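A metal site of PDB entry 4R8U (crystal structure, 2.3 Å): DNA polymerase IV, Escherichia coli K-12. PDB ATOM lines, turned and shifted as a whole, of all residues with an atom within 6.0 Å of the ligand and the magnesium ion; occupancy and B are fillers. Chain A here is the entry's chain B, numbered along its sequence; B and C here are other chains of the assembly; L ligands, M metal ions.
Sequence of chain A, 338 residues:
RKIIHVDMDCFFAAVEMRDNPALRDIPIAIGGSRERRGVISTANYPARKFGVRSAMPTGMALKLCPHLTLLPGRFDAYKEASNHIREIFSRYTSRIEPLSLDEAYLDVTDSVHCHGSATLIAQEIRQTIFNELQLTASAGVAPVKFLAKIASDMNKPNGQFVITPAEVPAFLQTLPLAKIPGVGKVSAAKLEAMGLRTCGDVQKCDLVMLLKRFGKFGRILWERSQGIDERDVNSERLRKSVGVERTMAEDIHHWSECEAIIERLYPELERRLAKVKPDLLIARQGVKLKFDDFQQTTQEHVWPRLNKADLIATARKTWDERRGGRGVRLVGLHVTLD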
ATOM      1  N   ASP A   7       1.689  18.267  26.172  1.00  0.00           N
ATOM      2  CA  ASP A   7       1.005  17.009  26.459  1.00  0.00           C
ATOM      3  C   ASP A   7       1.703  16.236  27.591  1.00  0.00           C
ATOM      4  O   ASP A   7       2.827  15.782  27.419  1.00  0.00           O
ATOM      5  CB  ASP A   7       0.935  16.153  25.170  1.00  0.00           C
ATOM      6  CG  ASP A   7      -0.203  15.119  25.180  1.00  0.00           C
ATOM      7  OD1 ASP A   7      -0.473  14.522  26.235  1.00  0.00           O
ATOM      8  OD2 ASP A   7      -0.819  14.883  24.110  1.00  0.00           O
ATOM      9  N   MET A   8       1.038  16.088  28.733  1.00  0.00           N
ATOM     10  CA  MET A   8       1.598  15.342  29.857  1.00  0.00           C
ATOM     11  C   MET A   8       1.779  13.863  29.515  1.00  0.00           C
ATOM     12  O   MET A   8       0.937  13.258  28.873  1.00  0.00           O
ATOM     13  CB  MET A   8       0.686  15.462  31.082  1.00  0.00           C
ATOM     14  CG  MET A   8       0.351  16.898  31.475  1.00  0.00           C
ATOM     15  SD  MET A   8       1.863  17.769  31.937  1.00  0.00           S
ATOM     16  CE  MET A   8       2.431  16.747  33.295  1.00  0.00           C
ATOM     17  N   ASP A   9       2.881  13.282  29.975  1.00  0.00           N
ATOM     18  CA  ASP A   9       3.173  11.877  29.691  1.00  0.00           C
ATOM     19  C   ASP A   9       2.447  10.940  30.653  1.00  0.00           C
ATOM     20  O   ASP A   9       2.485  11.173  31.873  1.00  0.00           O
ATOM     21  CB  ASP A   9       4.681  11.656  29.746  1.00  0.00           C
ATOM     22  CG  ASP A   9       5.436  12.592  28.803  1.00  0.00           C
ATOM     23  OD1 ASP A   9       4.932  12.853  27.694  1.00  0.00           O
ATOM     24  OD2 ASP A   9       6.519  13.083  29.180  1.00  0.00           O
ATOM     25  N   CYS A  10       1.784   9.915  30.115  1.00  0.00           N
ATOM     26  CA  CYS A  10       0.966   8.961  30.880  1.00  0.00           C
ATOM     27  C   CYS A  10       0.259   9.602  32.065  1.00  0.00           C
ATOM     28  O   CYS A  10       0.417   9.179  33.215  1.00  0.00           O
ATOM     29  CB  CYS A  10       1.830   7.804  31.397  1.00  0.00           C
ATOM     30  SG  CYS A  10       3.122   7.326  30.280  1.00  0.00           S
ATOM     31  N   PHE A  11      -0.528  10.638  31.770  1.00  0.00           N
ATOM     32  CA  PHE A  11      -0.942  11.609  32.771  1.00  0.00           C
ATOM     33  C   PHE A  11      -1.422  11.001  34.100  1.00  0.00           C
ATOM     34  O   PHE A  11      -0.856  11.343  35.136  1.00  0.00           O
ATOM     35  CB  PHE A  11      -2.026  12.520  32.196  1.00  0.00           C
ATOM     36  CG  PHE A  11      -2.458  13.614  33.135  1.00  0.00           C
ATOM     37  CD1 PHE A  11      -1.530  14.310  33.884  1.00  0.00           C
ATOM     38  CD2 PHE A  11      -3.804  13.944  33.260  1.00  0.00           C
ATOM     39  CE1 PHE A  11      -1.913  15.298  34.744  1.00  0.00           C
ATOM     40  CE2 PHE A  11      -4.206  14.943  34.118  1.00  0.00           C
ATOM     41  CZ  PHE A  11      -3.267  15.621  34.861  1.00  0.00           C
ATOM     42  N   PHE A  12      -2.420  10.115  34.075  1.00  0.00           N
ATOM     43  CA  PHE A  12      -2.951   9.539  35.316  1.00  0.00           C
ATOM     44  C   PHE A  12      -1.928   8.645  35.994  1.00  0.00           C
ATOM     45  O   PHE A  12      -1.788   8.678  37.217  1.00  0.00           O
ATOM     46  CB  PHE A  12      -4.221   8.709  35.087  1.00  0.00           C
ATOM     47  CG  PHE A  12      -5.430   9.501  34.694  1.00  0.00           C
ATOM     48  CD1 PHE A  12      -5.366  10.866  34.461  1.00  0.00           C
ATOM     49  CD2 PHE A  12      -6.653   8.854  34.550  1.00  0.00           C
ATOM     50  CE1 PHE A  12      -6.486  11.562  34.086  1.00  0.00           C
ATOM     51  CE2 PHE A  12      -7.778   9.561  34.184  1.00  0.00           C
ATOM     52  CZ  PHE A  12      -7.704  10.908  33.944  1.00  0.00           C
ATOM     53  N   ALA A  13      -1.252   7.811  35.211  1.00  0.00           N
ATOM     54  CA  ALA A  13      -0.316   6.851  35.798  1.00  0.00           C
ATOM     55  C   ALA A  13       0.922   7.549  36.372  1.00  0.00           C
ATOM     56  O   ALA A  13       1.518   7.049  37.328  1.00  0.00           O
ATOM     57  CB  ALA A  13       0.089   5.806  34.765  1.00  0.00           C
ATOM     58  N   ILE A  40      -9.297   0.172  30.719  1.00  0.00           N
ATOM     59  CA  ILE A  40      -8.108   0.921  31.108  1.00  0.00           C
ATOM     60  C   ILE A  40      -8.229   2.408  30.710  1.00  0.00           C
ATOM     61  O   ILE A  40      -8.435   2.708  29.532  1.00  0.00           O
ATOM     62  CB  ILE A  40      -6.842   0.339  30.452  1.00  0.00           C
ATOM     63  CG1 ILE A  40      -6.681  -1.161  30.778  1.00  0.00           C
ATOM     64  CG2 ILE A  40      -5.627   1.141  30.837  1.00  0.00           C
ATOM     65  CD1 ILE A  40      -6.701  -1.487  32.266  1.00  0.00           C
ATOM     66  N   SER A  41      -8.104   3.332  31.679  1.00  0.00           N
ATOM     67  CA  SER A  41      -8.022   4.750  31.348  1.00  0.00           C
ATOM     68  C   SER A  41      -6.662   5.051  30.745  1.00  0.00           C
ATOM     69  O   SER A  41      -6.554   5.702  29.707  1.00  0.00           O
ATOM     70  CB  SER A  41      -8.255   5.646  32.574  1.00  0.00           C
ATOM     71  OG  SER A  41      -9.584   6.127  32.659  1.00  0.00           O
ATOM     72  N   THR A  42      -5.628   4.582  31.429  1.00  0.00           N
ATOM     73  CA  THR A  42      -4.264   4.696  30.913  1.00  0.00           C
ATOM     74  C   THR A  42      -3.357   3.693  31.625  1.00  0.00           C
ATOM     75  O   THR A  42      -3.714   3.133  32.666  1.00  0.00           O
ATOM     76  CB  THR A  42      -3.717   6.141  31.084  1.00  0.00           C
ATOM     77  OG1 THR A  42      -2.566   6.315  30.256  1.00  0.00           O
ATOM     78  CG2 THR A  42      -3.338   6.404  32.523  1.00  0.00           C
ATOM     79  N   ALA A  43      -2.192   3.452  31.046  1.00  0.00           N
ATOM     80  CA  ALA A  43      -1.231   2.542  31.617  1.00  0.00           C
ATOM     81  C   ALA A  43       0.144   3.199  31.553  1.00  0.00           C
ATOM     82  O   ALA A  43       0.384   3.989  30.637  1.00  0.00           O
ATOM     83  CB  ALA A  43      -1.231   1.212  30.877  1.00  0.00           C
ATOM     84  N   TYR A  45       4.483   3.016  31.207  1.00  0.00           N
ATOM     85  CA  TYR A  45       5.313   2.401  30.163  1.00  0.00           C
ATOM     86  C   TYR A  45       5.712   0.940  30.372  1.00  0.00           C
ATOM     87  O   TYR A  45       5.768   0.186  29.401  1.00  0.00           O
ATOM     88  CB  TYR A  45       6.573   3.238  29.927  1.00  0.00           C
ATOM     89  CG  TYR A  45       6.340   4.294  28.880  1.00  0.00           C
ATOM     90  CD1 TYR A  45       6.494   4.016  27.526  1.00  0.00           C
ATOM     91  CD2 TYR A  45       5.920   5.567  29.237  1.00  0.00           C
ATOM     92  CE1 TYR A  45       6.259   4.990  26.562  1.00  0.00           C
ATOM     93  CE2 TYR A  45       5.686   6.546  28.293  1.00  0.00           C
ATOM     94  CZ  TYR A  45       5.852   6.256  26.961  1.00  0.00           C
ATOM     95  OH  TYR A  45       5.605   7.242  26.036  1.00  0.00           O
ATOM     96  N   ARG A  48       2.782  -0.721  29.070  1.00  0.00           N
ATOM     97  CA  ARG A  48       2.555  -0.539  27.633  1.00  0.00           C
ATOM     98  C   ARG A  48       3.385  -1.535  26.810  1.00  0.00           C
ATOM     99  O   ARG A  48       2.984  -1.948  25.719  1.00  0.00           O
ATOM    100  CB  ARG A  48       2.872   0.898  27.221  1.00  0.00           C
ATOM    101  CG  ARG A  48       1.887   1.922  27.800  1.00  0.00           C
ATOM    102  CD  ARG A  48       2.097   3.340  27.286  1.00  0.00           C
ATOM    103  NE  ARG A  48       1.185   4.259  27.948  1.00  0.00           N
ATOM    104  CZ  ARG A  48       1.019   5.535  27.617  1.00  0.00           C
ATOM    105  NH1 ARG A  48       1.720   6.079  26.621  1.00  0.00           N
ATOM    106  NH2 ARG A  48       0.150   6.279  28.300  1.00  0.00           N
ATOM    107  N   SER A  54      -4.902   2.480  26.541  1.00  0.00           N
ATOM    108  CA  SER A  54      -6.152   3.149  26.863  1.00  0.00           C
ATOM    109  C   SER A  54      -7.322   2.540  26.086  1.00  0.00           C
ATOM    110  O   SER A  54      -7.148   2.112  24.944  1.00  0.00           O
ATOM    111  CB  SER A  54      -6.046   4.649  26.552  1.00  0.00           C
ATOM    112  OG  SER A  54      -5.198   5.303  27.471  1.00  0.00           O
ATOM    113  N   ALA A  55      -8.486   2.478  26.732  1.00  0.00           N
ATOM    114  CA  ALA A  55      -9.765   2.030  26.138  1.00  0.00           C
ATOM    115  C   ALA A  55      -9.874   0.503  26.033  1.00  0.00           C
ATOM    116  O   ALA A  55     -10.939  -0.044  25.741  1.00  0.00           O
ATOM    117  CB  ALA A  55     -10.007   2.680  24.761  1.00  0.00           C
ATOM    118  N   SER A 100      -8.227  19.180  27.497  1.00  0.00           N
ATOM    119  CA  SER A 100      -8.564  18.229  28.542  1.00  0.00           C
ATOM    120  C   SER A 100      -7.698  18.585  29.731  1.00  0.00           C
ATOM    121  O   SER A 100      -6.969  19.569  29.687  1.00  0.00           O
ATOM    122  CB  SER A 100      -8.290  16.782  28.114  1.00  0.00           C
ATOM    123  OG  SER A 100      -6.895  16.582  27.933  1.00  0.00           O
ATOM    124  N   ASP A 102      -4.965  17.432  30.565  1.00  0.00           N
ATOM    125  CA  ASP A 102      -3.539  17.175  30.417  1.00  0.00           C
ATOM    126  C   ASP A 102      -2.874  17.835  29.208  1.00  0.00           C
ATOM    127  O   ASP A 102      -1.695  17.609  28.954  1.00  0.00           O
ATOM    128  CB  ASP A 102      -3.296  15.667  30.326  1.00  0.00           C
ATOM    129  CG  ASP A 102      -3.348  15.137  28.903  1.00  0.00           C
ATOM    130  OD1 ASP A 102      -4.341  15.393  28.177  1.00  0.00           O
ATOM    131  OD2 ASP A 102      -2.367  14.500  28.486  1.00  0.00           O
ATOM    132  N   GLU A 103      -3.626  18.611  28.440  1.00  0.00           N
ATOM    133  CA  GLU A 103      -3.021  19.226  27.266  1.00  0.00           C
ATOM    134  C   GLU A 103      -3.681  20.527  26.835  1.00  0.00           C
ATOM    135  O   GLU A 103      -4.864  20.766  27.107  1.00  0.00           O
ATOM    136  CB  GLU A 103      -3.004  18.232  26.090  1.00  0.00           C
ATOM    137  CG  GLU A 103      -4.341  17.635  25.733  1.00  0.00           C
ATOM    138  CD  GLU A 103      -4.208  16.389  24.851  1.00  0.00           C
ATOM    139  OE1 GLU A 103      -3.622  15.386  25.304  1.00  0.00           O
ATOM    140  OE2 GLU A 103      -4.702  16.426  23.694  1.00  0.00           O
ATOM    141  N   ASP A 153       3.780  14.178  19.737  1.00  0.00           N
ATOM    142  CA  ASP A 153       3.823  12.736  19.962  1.00  0.00           C
ATOM    143  C   ASP A 153       5.148  12.119  19.529  1.00  0.00           C
ATOM    144  O   ASP A 153       5.411  10.962  19.824  1.00  0.00           O
ATOM    145  CB  ASP A 153       2.679  12.046  19.236  1.00  0.00           C
ATOM    146  CG  ASP A 153       1.474  11.847  20.125  1.00  0.00           C
ATOM    147  OD1 ASP A 153       1.670  11.468  21.303  1.00  0.00           O
ATOM    148  OD2 ASP A 153       0.339  12.071  19.643  1.00  0.00           O
ATOM    149  N   LYS A 156       7.956  11.673  22.505  1.00  0.00           N
ATOM    150  CA  LYS A 156       7.346  11.371  23.785  1.00  0.00           C
ATOM    151  C   LYS A 156       7.969  10.064  24.303  1.00  0.00           C
ATOM    152  O   LYS A 156       8.241   9.165  23.520  1.00  0.00           O
ATOM    153  CB  LYS A 156       5.823  11.287  23.611  1.00  0.00           C
ATOM    154  CG  LYS A 156       5.015  10.873  24.819  1.00  0.00           C
ATOM    155  CD  LYS A 156       3.521  10.831  24.457  1.00  0.00           C
ATOM    156  CE  LYS A 156       2.930  12.241  24.325  1.00  0.00           C
ATOM    157  NZ  LYS A 156       2.668  12.894  25.655  1.00  0.00           N
ATOM    158  N   PRO A 157       8.225   9.961  25.614  1.00  0.00           N
ATOM    159  CA  PRO A 157       7.991  10.924  26.699  1.00  0.00           C
ATOM    160  C   PRO A 157       9.155  11.901  26.918  1.00  0.00           C
ATOM    161  O   PRO A 157      10.259  11.672  26.422  1.00  0.00           O
ATOM    162  CB  PRO A 157       7.831  10.021  27.927  1.00  0.00           C
ATOM    163  CG  PRO A 157       8.763   8.873  27.631  1.00  0.00           C
ATOM    164  CD  PRO A 157       8.793   8.700  26.123  1.00  0.00           C
ATOM    165  P    DA B   3     -17.534  -0.053  28.341  1.00  0.00           P
ATOM    166  OP1  DA B   3     -18.872  -0.580  28.670  1.00  0.00           O
ATOM    167  OP2  DA B   3     -17.334   0.701  27.086  1.00  0.00           O
ATOM    168  O5'  DA B   3     -17.016   0.910  29.513  1.00  0.00           O
ATOM    169  C5'  DA B   3     -16.726   0.384  30.805  1.00  0.00           C
ATOM    170  C4'  DA B   3     -16.638   1.505  31.840  1.00  0.00           C
ATOM    171  O4'  DA B   3     -15.437   2.303  31.606  1.00  0.00           O
ATOM    172  C3'  DA B   3     -17.789   2.485  31.809  1.00  0.00           C
ATOM    173  O3'  DA B   3     -17.976   3.020  33.091  1.00  0.00           O
ATOM    174  C2'  DA B   3     -17.308   3.563  30.848  1.00  0.00           C
ATOM    175  C1'  DA B   3     -15.803   3.592  31.109  1.00  0.00           C
ATOM    176  N9   DA B   3     -15.054   3.830  29.897  1.00  0.00           N
ATOM    177  C8   DA B   3     -15.348   3.347  28.653  1.00  0.00           C
ATOM    178  N7   DA B   3     -14.503   3.724  27.731  1.00  0.00           N
ATOM    179  C5   DA B   3     -13.593   4.505  28.418  1.00  0.00           C
ATOM    180  C6   DA B   3     -12.452   5.199  27.998  1.00  0.00           C
ATOM    181  N6   DA B   3     -12.026   5.210  26.739  1.00  0.00           N
ATOM    182  N1   DA B   3     -11.768   5.894  28.938  1.00  0.00           N
ATOM    183  C2   DA B   3     -12.202   5.878  30.198  1.00  0.00           C
ATOM    184  N3   DA B   3     -13.262   5.258  30.709  1.00  0.00           N
ATOM    185  C4   DA B   3     -13.918   4.592  29.759  1.00  0.00           C
ATOM    186  P    DG B   4     -19.291   3.856  33.428  1.00  0.00           P
ATOM    187  OP1  DG B   4     -19.673   3.404  34.773  1.00  0.00           O
ATOM    188  OP2  DG B   4     -20.250   3.746  32.306  1.00  0.00           O
ATOM    189  O5'  DG B   4     -18.815   5.385  33.406  1.00  0.00           O
ATOM    190  C5'  DG B   4     -17.751   5.834  34.230  1.00  0.00           C
ATOM    191  C4'  DG B   4     -17.358   7.224  33.815  1.00  0.00           C
ATOM    192  O4'  DG B   4     -16.507   7.160  32.642  1.00  0.00           O
ATOM    193  C3'  DG B   4     -18.528   8.128  33.422  1.00  0.00           C
ATOM    194  O3'  DG B   4     -18.318   9.436  33.907  1.00  0.00           O
ATOM    195  C2'  DG B   4     -18.477   8.088  31.900  1.00  0.00           C
ATOM    196  C1'  DG B   4     -16.985   8.074  31.708  1.00  0.00           C
ATOM    197  N9   DG B   4     -16.553   7.680  30.365  1.00  0.00           N
ATOM    198  C8   DG B   4     -17.191   6.823  29.494  1.00  0.00           C
ATOM    199  N7   DG B   4     -16.558   6.682  28.365  1.00  0.00           N
ATOM    200  C5   DG B   4     -15.446   7.519  28.488  1.00  0.00           C
ATOM    201  C6   DG B   4     -14.405   7.795  27.569  1.00  0.00           C
ATOM    202  O6   DG B   4     -14.237   7.338  26.424  1.00  0.00           O
ATOM    203  N1   DG B   4     -13.485   8.701  28.111  1.00  0.00           N
ATOM    204  C2   DG B   4     -13.572   9.261  29.370  1.00  0.00           C
ATOM    205  N2   DG B   4     -12.597  10.129  29.732  1.00  0.00           N
ATOM    206  N3   DG B   4     -14.545   9.003  30.218  1.00  0.00           N
ATOM    207  C4   DG B   4     -15.448   8.142  29.716  1.00  0.00           C
ATOM    208  P    DC C  16      -6.694  13.901  21.622  1.00  0.00           P
ATOM    209  OP1  DC C  16      -6.084  15.245  21.515  1.00  0.00           O
ATOM    210  OP2  DC C  16      -5.958  12.689  21.179  1.00  0.00           O
ATOM    211  O5'  DC C  16      -7.106  13.638  23.149  1.00  0.00           O
ATOM    212  C5'  DC C  16      -7.916  14.562  23.856  1.00  0.00           C
ATOM    213  C4'  DC C  16      -8.102  14.072  25.271  1.00  0.00           C
ATOM    214  O4'  DC C  16      -9.246  13.214  25.320  1.00  0.00           O
ATOM    215  C3'  DC C  16      -6.927  13.251  25.808  1.00  0.00           C
ATOM    216  O3'  DC C  16      -6.217  14.003  26.763  1.00  0.00           O
ATOM    217  C2'  DC C  16      -7.552  11.989  26.411  1.00  0.00           C
ATOM    218  C1'  DC C  16      -9.052  12.216  26.303  1.00  0.00           C
ATOM    219  N1   DC C  16      -9.799  11.030  25.852  1.00  0.00           N
ATOM    220  C2   DC C  16     -10.748  10.443  26.688  1.00  0.00           C
ATOM    221  O2   DC C  16     -10.939  10.928  27.807  1.00  0.00           O
ATOM    222  N3   DC C  16     -11.438   9.358  26.239  1.00  0.00           N
ATOM    223  C4   DC C  16     -11.212   8.872  25.004  1.00  0.00           C
ATOM    224  N4   DC C  16     -11.910   7.814  24.600  1.00  0.00           N
ATOM    225  C5   DC C  16     -10.248   9.464  24.145  1.00  0.00           C
ATOM    226  C6   DC C  16      -9.569  10.531  24.599  1.00  0.00           C
HETATM  227  O1  LIG L   1      -9.409   8.218  30.687  1.00  0.00           O
HETATM  228  O2  LIG L   1      -9.086   6.267  26.416  1.00  0.00           O
HETATM  229  C1  LIG L   1      -8.626   7.173  27.327  1.00  0.00           C
HETATM  230  C2  LIG L   1      -7.487   8.089  26.985  1.00  0.00           C
HETATM  231  C3  LIG L   1      -7.059   8.975  27.965  1.00  0.00           C
HETATM  232  C4  LIG L   1      -6.789   8.022  25.647  1.00  0.00           C
HETATM  233  N1  LIG L   1      -9.201   7.273  28.546  1.00  0.00           N
HETATM  234  C5  LIG L   1      -8.774   8.160  29.474  1.00  0.00           C
HETATM  235  N2  LIG L   1      -7.764   9.112  29.193  1.00  0.00           N
HETATM  236  C6  LIG L   1      -7.045   9.693  30.355  1.00  0.00           C
HETATM  237  C7  LIG L   1      -5.822   8.932  30.791  1.00  0.00           C
HETATM  238  C8  LIG L   1      -4.658   9.772  30.291  1.00  0.00           C
HETATM  239  O3  LIG L   1      -3.574   9.731  31.226  1.00  0.00           O
HETATM  240  O4  LIG L   1      -6.646  11.008  29.969  1.00  0.00           O
HETATM  241  C9  LIG L   1      -5.224  11.164  30.111  1.00  0.00           C
HETATM  242  C10 LIG L   1      -4.676  11.917  28.906  1.00  0.00           C
HETATM  243  O5  LIG L   1      -4.799  11.151  27.691  1.00  0.00           O
HETATM  244  P1  LIG L   1      -3.527  10.848  26.707  1.00  0.00           P
HETATM  245  O6  LIG L   1      -2.607  12.080  26.764  1.00  0.00           O
HETATM  246  O7  LIG L   1      -4.133  10.463  25.364  1.00  0.00           O
HETATM  247  N3  LIG L   1      -2.687   9.604  27.299  1.00  0.00           N
HETATM  248  P2  LIG L   1      -1.523   9.661  28.442  1.00  0.00           P
HETATM  249  O8  LIG L   1      -1.677   8.588  29.485  1.00  0.00           O
HETATM  250  O9  LIG L   1      -1.283  11.041  28.999  1.00  0.00           O
HETATM  251  O10 LIG L   1      -0.268   9.071  27.603  1.00  0.00           O
HETATM  252  P3  LIG L   1       0.722   9.956  26.658  1.00  0.00           P
HETATM  253  O11 LIG L   1      -0.084  11.175  26.309  1.00  0.00           O
HETATM  254  O12 LIG L   1       1.901  10.164  27.535  1.00  0.00           O
HETATM  255  O13 LIG L   1       1.017   8.938  25.584  1.00  0.00           O
HETATM  256 MG    MG M   1      -0.964  12.801  27.607  1.00  0.00          MG
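Three residues have an atom within 4 Å of the magnesium ion: Asp 7, Met 8 and Asp 102. Along chain A the residues within 4 Å of the magnesium ion span positions 7 to 102.
O6 of the ligand is bound to the magnesium ion (2.0 Å). OD1 of Asp 7 is bound to the magnesium ion, at 2.3 Å. The magnesium ion is bound by O11 of the ligand (2.3 Å). O9 of the ligand is bound to the magnesium ion (2.3 Å). The backbone carbonyl oxygen (O) of Met 8 is bound to the magnesium ion, at 2.3 Å. OD2 of Asp 102 binds the magnesium ion. The magnesium ion has six donor atoms within binding distance.
O3' of DC 16 of chain C sits close to an oxygen (O5) of the ligand, at 3.3 Å. Asp 9 touches the ligand. Ser 54 touches the ligand (CB to O2, 3.4 Å). Ala 55 touches the ligand. OE1 of Glu 103 touches O6 of the ligand, 3.8 Å away. N2 of DG 4 of chain B touches O1 of the ligand, 3.8 Å away. Hydrophobic or aromatic side chains that line the ligand: Phe 11 and Phe 12. 17 residues have an atom within 4 Å of the ligand: Asp 7, Met 8, Asp 9, Cys 10, Phe 11, Phe 12, Ser 41, Thr 42, Arg 48, Ser 54, Ala 55, Asp 102, Glu 103, Lys 156, DA 3 of chain B, DG 4 of chain B and DC 16 of chain C. The nearest printed residue that does not touch the ligand is Ile 40 (4.7 Å).
O3' of DC 16 of chain C sits close to OD1 of Asp 102. OD1 of Asp 102 is in hydrogen-bond range of OG of Ser 100 (2.8 Å). The guanidinium group (NH2) of Arg 48 sits at hydrogen-bond distance from the side-chain sulfur (SG) of Cys 10. O of Ser 41 sits at hydrogen-bond distance from OG of Ser 54 (2.6 Å). The side-chain carboxylate of Asp 9 is in salt-bridge range of the side-chain amino group of Lys 156 (3.0 Å). N2 of DG 4 of chain B sits close to O2 of DC 16 of chain C, 2.7 Å away. The side-chain hydroxyl (OG) of Ser 100 is in hydrogen-bond range of O3' of DC 16 of chain C. The backbone NH of Ala 55 is in hydrogen-bond range of the backbone carbonyl oxygen of Ile 40, at 2.8 Å.
OG1 of Thr 42 is in hydrogen-bond range of O8 of the ligand, 2.6 Å away. An oxygen (O12) of the ligand is in hydrogen-bond range of the backbone NH of Cys 10 (2.6 Å). N1 of the ligand sits at hydrogen-bond distance from O of Ser 41, 3.3 Å away. The side-chain hydroxyl (OG) of Ser 41 sits at hydrogen-bond distance from an oxygen (O1) of the ligand (2.9 Å). N of Phe 11 lies within hydrogen-bond range of O3 of the ligand, 3.2 Å away. The guanidinium group (NH1) of Arg 48 is in salt-bridge range of an oxygen (O13) of the ligand, at 3.1 Å. N1 of DA 3 of chain B sits at hydrogen-bond distance from a nitrogen (N1) of the ligand (2.9 Å). O3 of the ligand is in hydrogen-bond range of N of Phe 12 (3.1 Å). NZ of Lys 156 is in salt-bridge range of O12 of the ligand (3.4 Å).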
